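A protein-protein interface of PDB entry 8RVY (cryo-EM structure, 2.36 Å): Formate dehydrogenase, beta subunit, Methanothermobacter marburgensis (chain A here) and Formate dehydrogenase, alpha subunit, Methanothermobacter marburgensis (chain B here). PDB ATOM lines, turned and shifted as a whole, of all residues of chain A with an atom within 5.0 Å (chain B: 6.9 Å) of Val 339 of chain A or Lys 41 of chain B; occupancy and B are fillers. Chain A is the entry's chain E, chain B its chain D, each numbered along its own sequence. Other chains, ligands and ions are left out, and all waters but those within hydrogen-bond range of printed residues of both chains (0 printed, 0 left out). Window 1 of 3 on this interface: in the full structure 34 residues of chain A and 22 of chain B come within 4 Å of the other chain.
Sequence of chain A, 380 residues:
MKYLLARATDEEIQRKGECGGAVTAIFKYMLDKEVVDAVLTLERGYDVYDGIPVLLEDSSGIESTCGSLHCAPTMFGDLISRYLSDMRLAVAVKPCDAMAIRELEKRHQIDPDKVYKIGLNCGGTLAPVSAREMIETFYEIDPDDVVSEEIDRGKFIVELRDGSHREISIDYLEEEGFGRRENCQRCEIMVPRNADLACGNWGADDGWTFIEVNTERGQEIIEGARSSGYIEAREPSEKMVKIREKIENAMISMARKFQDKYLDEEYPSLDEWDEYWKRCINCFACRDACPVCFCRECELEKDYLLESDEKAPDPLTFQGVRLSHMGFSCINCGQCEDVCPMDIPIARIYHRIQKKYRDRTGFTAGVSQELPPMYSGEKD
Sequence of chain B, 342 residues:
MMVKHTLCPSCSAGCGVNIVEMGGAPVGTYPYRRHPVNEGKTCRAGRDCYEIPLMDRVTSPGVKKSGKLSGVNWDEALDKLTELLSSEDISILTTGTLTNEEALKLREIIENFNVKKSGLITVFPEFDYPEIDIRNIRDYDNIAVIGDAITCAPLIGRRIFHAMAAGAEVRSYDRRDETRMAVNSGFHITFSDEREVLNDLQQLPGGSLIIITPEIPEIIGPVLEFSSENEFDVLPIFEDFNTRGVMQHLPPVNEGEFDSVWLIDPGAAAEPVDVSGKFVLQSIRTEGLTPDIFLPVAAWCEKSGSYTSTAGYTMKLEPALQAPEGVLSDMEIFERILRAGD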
ATOM      1  N   ALA A 285     -12.118  -3.087  28.143  1.00  0.00           N
ATOM      2  CA  ALA A 285     -13.072  -2.699  27.110  1.00  0.00           C
ATOM      3  C   ALA A 285     -13.324  -3.844  26.138  1.00  0.00           C
ATOM      4  O   ALA A 285     -14.450  -4.025  25.663  1.00  0.00           O
ATOM      5  CB  ALA A 285     -12.571  -1.461  26.370  1.00  0.00           C
ATOM      6  N   CYS A 286     -12.286  -4.622  25.825  1.00  0.00           N
ATOM      7  CA  CYS A 286     -12.453  -5.780  24.956  1.00  0.00           C
ATOM      8  C   CYS A 286     -13.417  -6.787  25.567  1.00  0.00           C
ATOM      9  O   CYS A 286     -14.301  -7.314  24.884  1.00  0.00           O
ATOM     10  CB  CYS A 286     -11.096  -6.430  24.703  1.00  0.00           C
ATOM     11  SG  CYS A 286     -10.116  -6.686  26.199  1.00  0.00           S
ATOM     12  N   ALA A 289     -17.038  -5.307  25.492  1.00  0.00           N
ATOM     13  CA  ALA A 289     -17.628  -5.248  24.161  1.00  0.00           C
ATOM     14  C   ALA A 289     -17.923  -6.628  23.594  1.00  0.00           C
ATOM     15  O   ALA A 289     -18.833  -6.766  22.772  1.00  0.00           O
ATOM     16  CB  ALA A 289     -16.702  -4.493  23.210  1.00  0.00           C
ATOM     17  N   GLN A 335     -15.586  -6.468  17.702  1.00  0.00           N
ATOM     18  CA  GLN A 335     -15.938  -5.440  18.677  1.00  0.00           C
ATOM     19  C   GLN A 335     -14.803  -5.197  19.665  1.00  0.00           C
ATOM     20  O   GLN A 335     -14.521  -4.047  20.029  1.00  0.00           O
ATOM     21  CB  GLN A 335     -17.215  -5.834  19.416  1.00  0.00           C
ATOM     22  CG  GLN A 335     -18.436  -5.949  18.527  1.00  0.00           C
ATOM     23  CD  GLN A 335     -18.830  -4.632  17.911  1.00  0.00           C
ATOM     24  OE1 GLN A 335     -18.866  -3.608  18.587  1.00  0.00           O
ATOM     25  NE2 GLN A 335     -19.122  -4.645  16.620  1.00  0.00           N
ATOM     26  N   CYS A 336     -14.143  -6.267  20.107  1.00  0.00           N
ATOM     27  CA  CYS A 336     -13.035  -6.130  21.044  1.00  0.00           C
ATOM     28  C   CYS A 336     -11.925  -5.273  20.453  1.00  0.00           C
ATOM     29  O   CYS A 336     -11.383  -4.389  21.122  1.00  0.00           O
ATOM     30  CB  CYS A 336     -12.499  -7.513  21.416  1.00  0.00           C
ATOM     31  SG  CYS A 336     -11.977  -8.516  19.999  1.00  0.00           S
ATOM     32  N   GLU A 337     -11.567  -5.530  19.197  1.00  0.00           N
ATOM     33  CA  GLU A 337     -10.565  -4.712  18.531  1.00  0.00           C
ATOM     34  C   GLU A 337     -11.086  -3.305  18.262  1.00  0.00           C
ATOM     35  O   GLU A 337     -10.312  -2.344  18.285  1.00  0.00           O
ATOM     36  CB  GLU A 337     -10.135  -5.388  17.230  1.00  0.00           C
ATOM     37  CG  GLU A 337      -9.114  -4.608  16.439  1.00  0.00           C
ATOM     38  CD  GLU A 337      -8.323  -5.475  15.482  1.00  0.00           C
ATOM     39  OE1 GLU A 337      -8.442  -6.714  15.551  1.00  0.00           O
ATOM     40  OE2 GLU A 337      -7.571  -4.916  14.658  1.00  0.00           O
ATOM     41  N   ASP A 338     -12.387  -3.167  18.010  1.00  0.00           N
ATOM     42  CA  ASP A 338     -12.966  -1.849  17.777  1.00  0.00           C
ATOM     43  C   ASP A 338     -12.796  -0.943  18.986  1.00  0.00           C
ATOM     44  O   ASP A 338     -12.444   0.232  18.843  1.00  0.00           O
ATOM     45  CB  ASP A 338     -14.451  -1.981  17.441  1.00  0.00           C
ATOM     46  CG  ASP A 338     -14.711  -2.088  15.961  1.00  0.00           C
ATOM     47  OD1 ASP A 338     -13.738  -2.138  15.180  1.00  0.00           O
ATOM     48  OD2 ASP A 338     -15.897  -2.123  15.575  1.00  0.00           O
ATOM     49  N   VAL A 339     -13.055  -1.465  20.190  1.00  0.00           N
ATOM     50  CA  VAL A 339     -13.115  -0.613  21.373  1.00  0.00           C
ATOM     51  C   VAL A 339     -11.780  -0.485  22.097  1.00  0.00           C
ATOM     52  O   VAL A 339     -11.696   0.264  23.077  1.00  0.00           O
ATOM     53  CB  VAL A 339     -14.177  -1.125  22.367  1.00  0.00           C
ATOM     54  CG1 VAL A 339     -15.545  -1.136  21.718  1.00  0.00           C
ATOM     55  CG2 VAL A 339     -13.816  -2.505  22.882  1.00  0.00           C
ATOM     56  N   CYS A 340     -10.739  -1.172  21.652  1.00  0.00           N
ATOM     57  CA  CYS A 340      -9.488  -1.174  22.402  1.00  0.00           C
ATOM     58  C   CYS A 340      -8.856   0.211  22.374  1.00  0.00           C
ATOM     59  O   CYS A 340      -8.512   0.698  21.290  1.00  0.00           O
ATOM     60  CB  CYS A 340      -8.520  -2.203  21.828  1.00  0.00           C
ATOM     61  SG  CYS A 340      -6.960  -2.351  22.739  1.00  0.00           S
ATOM     62  N   PRO A 341      -8.663   0.875  23.519  1.00  0.00           N
ATOM     63  CA  PRO A 341      -8.036   2.205  23.492  1.00  0.00           C
ATOM     64  C   PRO A 341      -6.585   2.183  23.062  1.00  0.00           C
ATOM     65  O   PRO A 341      -6.029   3.251  22.784  1.00  0.00           O
ATOM     66  CB  PRO A 341      -8.173   2.694  24.941  1.00  0.00           C
ATOM     67  CG  PRO A 341      -9.153   1.796  25.583  1.00  0.00           C
ATOM     68  CD  PRO A 341      -9.069   0.497  24.882  1.00  0.00           C
ATOM     69  N   ASP A 343      -5.342   0.135  20.493  1.00  0.00           N
ATOM     70  CA  ASP A 343      -5.207  -0.319  19.110  1.00  0.00           C
ATOM     71  C   ASP A 343      -4.434  -1.633  19.031  1.00  0.00           C
ATOM     72  O   ASP A 343      -3.505  -1.791  18.237  1.00  0.00           O
ATOM     73  CB  ASP A 343      -4.544   0.754  18.246  1.00  0.00           C
ATOM     74  CG  ASP A 343      -5.375   2.008  18.142  1.00  0.00           C
ATOM     75  OD1 ASP A 343      -6.614   1.898  18.097  1.00  0.00           O
ATOM     76  OD2 ASP A 343      -4.789   3.106  18.112  1.00  0.00           O
ATOM     77  N   CYS B  15     -13.679  12.445  25.227  1.00  0.00           N
ATOM     78  CA  CYS B  15     -14.258  11.212  24.709  1.00  0.00           C
ATOM     79  C   CYS B  15     -15.780  11.250  24.763  1.00  0.00           C
ATOM     80  O   CYS B  15     -16.373  11.726  25.733  1.00  0.00           O
ATOM     81  CB  CYS B  15     -13.738  10.016  25.504  1.00  0.00           C
ATOM     82  SG  CYS B  15     -11.953   9.788  25.418  1.00  0.00           S
ATOM     83  N   GLY B  16     -16.411  10.741  23.711  1.00  0.00           N
ATOM     84  CA  GLY B  16     -17.852  10.610  23.656  1.00  0.00           C
ATOM     85  C   GLY B  16     -18.307   9.207  24.017  1.00  0.00           C
ATOM     86  O   GLY B  16     -17.620   8.230  23.748  1.00  0.00           O
ATOM     87  N   VAL B  17     -19.486   9.122  24.631  1.00  0.00           N
ATOM     88  CA  VAL B  17     -20.064   7.847  25.038  1.00  0.00           C
ATOM     89  C   VAL B  17     -21.572   7.940  24.877  1.00  0.00           C
ATOM     90  O   VAL B  17     -22.153   9.017  25.003  1.00  0.00           O
ATOM     91  CB  VAL B  17     -19.692   7.490  26.499  1.00  0.00           C
ATOM     92  CG1 VAL B  17     -18.235   7.122  26.599  1.00  0.00           C
ATOM     93  CG2 VAL B  17     -20.000   8.645  27.429  1.00  0.00           C
ATOM     94  N   PRO B  31     -20.876   2.162  22.781  1.00  0.00           N
ATOM     95  CA  PRO B  31     -19.813   2.884  22.073  1.00  0.00           C
ATOM     96  C   PRO B  31     -20.351   4.027  21.227  1.00  0.00           C
ATOM     97  O   PRO B  31     -21.339   3.886  20.506  1.00  0.00           O
ATOM     98  CB  PRO B  31     -19.157   1.805  21.203  1.00  0.00           C
ATOM     99  CG  PRO B  31     -19.901   0.549  21.443  1.00  0.00           C
ATOM    100  CD  PRO B  31     -20.719   0.707  22.659  1.00  0.00           C
ATOM    101  N   TYR B  32     -19.671   5.167  21.318  1.00  0.00           N
ATOM    102  CA  TYR B  32     -19.950   6.335  20.487  1.00  0.00           C
ATOM    103  C   TYR B  32     -18.875   6.382  19.403  1.00  0.00           C
ATOM    104  O   TYR B  32     -17.905   7.132  19.478  1.00  0.00           O
ATOM    105  CB  TYR B  32     -19.974   7.591  21.354  1.00  0.00           C
ATOM    106  CG  TYR B  32     -20.477   8.855  20.693  1.00  0.00           C
ATOM    107  CD1 TYR B  32     -20.739   8.913  19.333  1.00  0.00           C
ATOM    108  CD2 TYR B  32     -20.680  10.001  21.444  1.00  0.00           C
ATOM    109  CE1 TYR B  32     -21.189  10.079  18.745  1.00  0.00           C
ATOM    110  CE2 TYR B  32     -21.125  11.165  20.868  1.00  0.00           C
ATOM    111  CZ  TYR B  32     -21.381  11.201  19.519  1.00  0.00           C
ATOM    112  OH  TYR B  32     -21.830  12.365  18.948  1.00  0.00           O
ATOM    113  N   ARG B  33     -19.066   5.557  18.374  1.00  0.00           N
ATOM    114  CA  ARG B  33     -18.042   5.399  17.347  1.00  0.00           C
ATOM    115  C   ARG B  33     -17.858   6.667  16.527  1.00  0.00           C
ATOM    116  O   ARG B  33     -16.748   6.943  16.057  1.00  0.00           O
ATOM    117  CB  ARG B  33     -18.405   4.238  16.427  1.00  0.00           C
ATOM    118  CG  ARG B  33     -18.064   2.877  16.981  1.00  0.00           C
ATOM    119  CD  ARG B  33     -18.648   1.774  16.120  1.00  0.00           C
ATOM    120  NE  ARG B  33     -18.372   0.454  16.671  1.00  0.00           N
ATOM    121  CZ  ARG B  33     -19.195  -0.229  17.454  1.00  0.00           C
ATOM    122  NH1 ARG B  33     -20.385   0.241  17.790  1.00  0.00           N
ATOM    123  NH2 ARG B  33     -18.816  -1.417  17.912  1.00  0.00           N
ATOM    124  N   VAL B  37     -12.797  12.163  18.805  1.00  0.00           N
ATOM    125  CA  VAL B  37     -11.728  12.144  19.799  1.00  0.00           C
ATOM    126  C   VAL B  37     -11.268  10.716  20.059  1.00  0.00           C
ATOM    127  O   VAL B  37     -10.069  10.419  20.036  1.00  0.00           O
ATOM    128  CB  VAL B  37     -12.188  12.834  21.097  1.00  0.00           C
ATOM    129  CG1 VAL B  37     -11.244  12.506  22.245  1.00  0.00           C
ATOM    130  CG2 VAL B  37     -12.273  14.328  20.899  1.00  0.00           C
ATOM    131  N   ASN B  38     -12.214   9.806  20.300  1.00  0.00           N
ATOM    132  CA  ASN B  38     -11.887   8.445  20.695  1.00  0.00           C
ATOM    133  C   ASN B  38     -12.423   7.375  19.760  1.00  0.00           C
ATOM    134  O   ASN B  38     -11.892   6.262  19.770  1.00  0.00           O
ATOM    135  CB  ASN B  38     -12.410   8.161  22.110  1.00  0.00           C
ATOM    136  CG  ASN B  38     -13.903   8.348  22.229  1.00  0.00           C
ATOM    137  OD1 ASN B  38     -14.473   9.257  21.636  1.00  0.00           O
ATOM    138  ND2 ASN B  38     -14.543   7.493  23.008  1.00  0.00           N
ATOM    139  N   GLU B  39     -13.449   7.670  18.964  1.00  0.00           N
ATOM    140  CA  GLU B  39     -14.005   6.709  18.012  1.00  0.00           C
ATOM    141  C   GLU B  39     -14.600   5.498  18.725  1.00  0.00           C
ATOM    142  O   GLU B  39     -14.453   4.360  18.281  1.00  0.00           O
ATOM    143  CB  GLU B  39     -12.948   6.271  16.998  1.00  0.00           C
ATOM    144  CG  GLU B  39     -12.306   7.417  16.247  1.00  0.00           C
ATOM    145  CD  GLU B  39     -10.826   7.207  16.022  1.00  0.00           C
ATOM    146  OE1 GLU B  39     -10.109   6.913  16.999  1.00  0.00           O
ATOM    147  OE2 GLU B  39     -10.376   7.337  14.865  1.00  0.00           O
ATOM    148  N   GLY B  40     -15.288   5.747  19.836  1.00  0.00           N
ATOM    149  CA  GLY B  40     -15.940   4.696  20.582  1.00  0.00           C
ATOM    150  C   GLY B  40     -15.054   3.951  21.550  1.00  0.00           C
ATOM    151  O   GLY B  40     -15.537   3.030  22.219  1.00  0.00           O
ATOM    152  N   LYS B  41     -13.781   4.309  21.648  1.00  0.00           N
ATOM    153  CA  LYS B  41     -12.883   3.701  22.615  1.00  0.00           C
ATOM    154  C   LYS B  41     -12.940   4.478  23.921  1.00  0.00           C
ATOM    155  O   LYS B  41     -13.006   5.709  23.921  1.00  0.00           O
ATOM    156  CB  LYS B  41     -11.454   3.667  22.074  1.00  0.00           C
ATOM    157  CG  LYS B  41     -11.320   2.915  20.769  1.00  0.00           C
ATOM    158  CD  LYS B  41     -10.076   3.310  20.017  1.00  0.00           C
ATOM    159  CE  LYS B  41     -10.020   2.655  18.655  1.00  0.00           C
ATOM    160  NZ  LYS B  41      -9.667   1.216  18.738  1.00  0.00           N
ATOM    161  N   THR B  42     -12.937   3.752  25.034  1.00  0.00           N
ATOM    162  CA  THR B  42     -12.957   4.371  26.349  1.00  0.00           C
ATOM    163  C   THR B  42     -12.132   3.538  27.314  1.00  0.00           C
ATOM    164  O   THR B  42     -11.962   2.333  27.129  1.00  0.00           O
ATOM    165  CB  THR B  42     -14.383   4.515  26.901  1.00  0.00           C
ATOM    166  OG1 THR B  42     -15.047   3.251  26.864  1.00  0.00           O
ATOM    167  CG2 THR B  42     -15.175   5.517  26.099  1.00  0.00           C
ATOM    168  N   CYS B  43     -11.620   4.199  28.346  1.00  0.00           N
ATOM    169  CA  CYS B  43     -10.998   3.510  29.460  1.00  0.00           C
ATOM    170  C   CYS B  43     -12.081   3.056  30.434  1.00  0.00           C
ATOM    171  O   CYS B  43     -13.272   3.286  30.228  1.00  0.00           O
ATOM    172  CB  CYS B  43      -9.976   4.417  30.139  1.00  0.00           C
ATOM    173  SG  CYS B  43     -10.695   5.800  31.049  1.00  0.00           S
ATOM    174  N   ARG B  47     -16.495   3.908  30.845  1.00  0.00           N
ATOM    175  CA  ARG B  47     -17.572   2.934  30.769  1.00  0.00           C
ATOM    176  C   ARG B  47     -18.342   2.795  32.074  1.00  0.00           C
ATOM    177  O   ARG B  47     -19.359   2.095  32.100  1.00  0.00           O
ATOM    178  CB  ARG B  47     -17.016   1.570  30.350  1.00  0.00           C
ATOM    179  CG  ARG B  47     -17.129   1.309  28.861  1.00  0.00           C
ATOM    180  CD  ARG B  47     -16.232   0.177  28.412  1.00  0.00           C
ATOM    181  NE  ARG B  47     -14.819   0.496  28.568  1.00  0.00           N
ATOM    182  CZ  ARG B  47     -13.988  -0.099  29.414  1.00  0.00           C
ATOM    183  NH1 ARG B  47     -14.392  -1.055  30.232  1.00  0.00           N
ATOM    184  NH2 ARG B  47     -12.716   0.278  29.442  1.00  0.00           N
ATOM    185  N   LEU B 155      -6.793   8.056  26.255  1.00  0.00           N
ATOM    186  CA  LEU B 155      -7.118   8.216  24.845  1.00  0.00           C
ATOM    187  C   LEU B 155      -6.270   9.272  24.147  1.00  0.00           C
ATOM    188  O   LEU B 155      -6.332   9.373  22.919  1.00  0.00           O
ATOM    189  CB  LEU B 155      -8.605   8.540  24.689  1.00  0.00           C
ATOM    190  CG  LEU B 155      -9.515   7.323  24.482  1.00  0.00           C
ATOM    191  CD1 LEU B 155      -9.129   6.557  23.229  1.00  0.00           C
ATOM    192  CD2 LEU B 155      -9.491   6.396  25.689  1.00  0.00           C
ATOM    193  N   ARG B 158      -3.109   7.087  23.462  1.00  0.00           N
ATOM    194  CA  ARG B 158      -3.326   6.382  22.204  1.00  0.00           C
ATOM    195  C   ARG B 158      -2.720   7.151  21.032  1.00  0.00           C
ATOM    196  O   ARG B 158      -2.040   6.574  20.173  1.00  0.00           O
ATOM    197  CB  ARG B 158      -4.826   6.169  22.000  1.00  0.00           C
ATOM    198  CG  ARG B 158      -5.232   5.849  20.582  1.00  0.00           C
ATOM    199  CD  ARG B 158      -6.681   5.441  20.506  1.00  0.00           C
ATOM    200  NE  ARG B 158      -7.061   5.078  19.147  1.00  0.00           N
ATOM    201  CZ  ARG B 158      -7.802   5.823  18.338  1.00  0.00           C
ATOM    202  NH1 ARG B 158      -8.288   6.992  18.719  1.00  0.00           N
ATOM    203  NH2 ARG B 158      -8.067   5.380  17.114  1.00  0.00           N
ATOM    204  N   HIS B 162       0.265   6.357  18.329  1.00  0.00           N
ATOM    205  CA  HIS B 162       0.203   6.574  16.886  1.00  0.00           C
ATOM    206  C   HIS B 162       1.412   7.364  16.405  1.00  0.00           C
ATOM    207  O   HIS B 162       2.034   7.023  15.394  1.00  0.00           O
ATOM    208  CB  HIS B 162      -1.083   7.311  16.513  1.00  0.00           C
ATOM    209  CG  HIS B 162      -2.320   6.486  16.655  1.00  0.00           C
ATOM    210  ND1 HIS B 162      -3.584   7.018  16.533  1.00  0.00           N
ATOM    211  CD2 HIS B 162      -2.490   5.168  16.909  1.00  0.00           C
ATOM    212  CE1 HIS B 162      -4.480   6.065  16.706  1.00  0.00           C
ATOM    213  NE2 HIS B 162      -3.842   4.933  16.938  1.00  0.00           N
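The backbone carbonyl oxygen (O) of Thr 42 of chain B lies within hydrogen-bond range of the guanidinium group (NH2) of Arg 47 of chain B. The backbone NH (N) of Asp 343 of chain A sits close to the side-chain sulfur (SG) of Cys 340 of chain A, at 3.7 Å. The side-chain amide nitrogen of Asn 38 of chain B is in hydrogen-bond range of the backbone carbonyl oxygen of Lys 41 of chain B, at 2.5 Å. NH2 of Arg 47 of chain B sits close to O of Cys 43 of chain B, 3.2 Å away. The side-chain carboxylate (OE1) of Glu 39 of chain B is in salt-bridge range of the guanidinium group (NH1) of Arg 158 of chain B (2.5 Å).
Among the printed residues, merely in contact across the chains: Ala 285 of chain A with Thr 42 of chain B (3.9 Å), Ala 285 of chain A with Arg 47 of chain B (3.5 Å), Glu 337 of chain A with Lys 41 of chain B (3.6 Å), Val 339 of chain A with Lys 41 of chain B (3.5 Å), Pro 341 of chain A with Lys 41 of chain B (3.98 Å), Pro 341 of chain A with Thr 42 of chain B (3.3 Å) and Pro 341 of chain A with Arg 158 of chain B (3.2 Å).
The side-chain carboxylate (OD2) of Asp 343 of chain A lies within salt-bridge range of the guanidinium group (NE) of Arg 158 of chain B (3.2 Å). The side-chain amide nitrogen of Gln 335 of chain A sits close to the guanidinium group of Arg 33 of chain B (3.5 Å). OD1 of Asp 343 of chain A lies within salt-bridge range of NZ of Lys 41 of chain B, at 3.2 Å. O of Cys 340 of chain A sits at hydrogen-bond distance from NZ of Lys 41 of chain B (2.8 Å). O of Asp 338 of chain A is in hydrogen-bond range of NZ of Lys 41 of chain B, at 2.9 Å. NE2 of His 162 of chain B lies close to OD2 of Asp 343 of chain A, 2.4 Å away. The side-chain carboxylate (OD2) of Asp 338 of chain A lies within salt-bridge range of the guanidinium group (NE) of Arg 33 of chain B (3.7 Å).
Val 339 of chain A touches just one residue of chain B: Lys 41. Of chain A, only Glu 337, Asp 338, Val 339, Cys 340, Pro 341 and Asp 343 come within 4 Å of Lys 41 of chain B. Of the printed residues of chain B, Pro 341 of chain A touches Lys 41 (3.98 Å), Thr 42 (3.3 Å) and Arg 158 (3.2 Å). Of the printed residues of chain B, Asp 338 of chain A touches Arg 33 and Lys 41. Leu 155 of chain B touches none of the printed residues of chain A. The nearest printed residue of chain A that does not touch Lys 41 of chain B is Cys 336 of chain A (6.3 Å).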
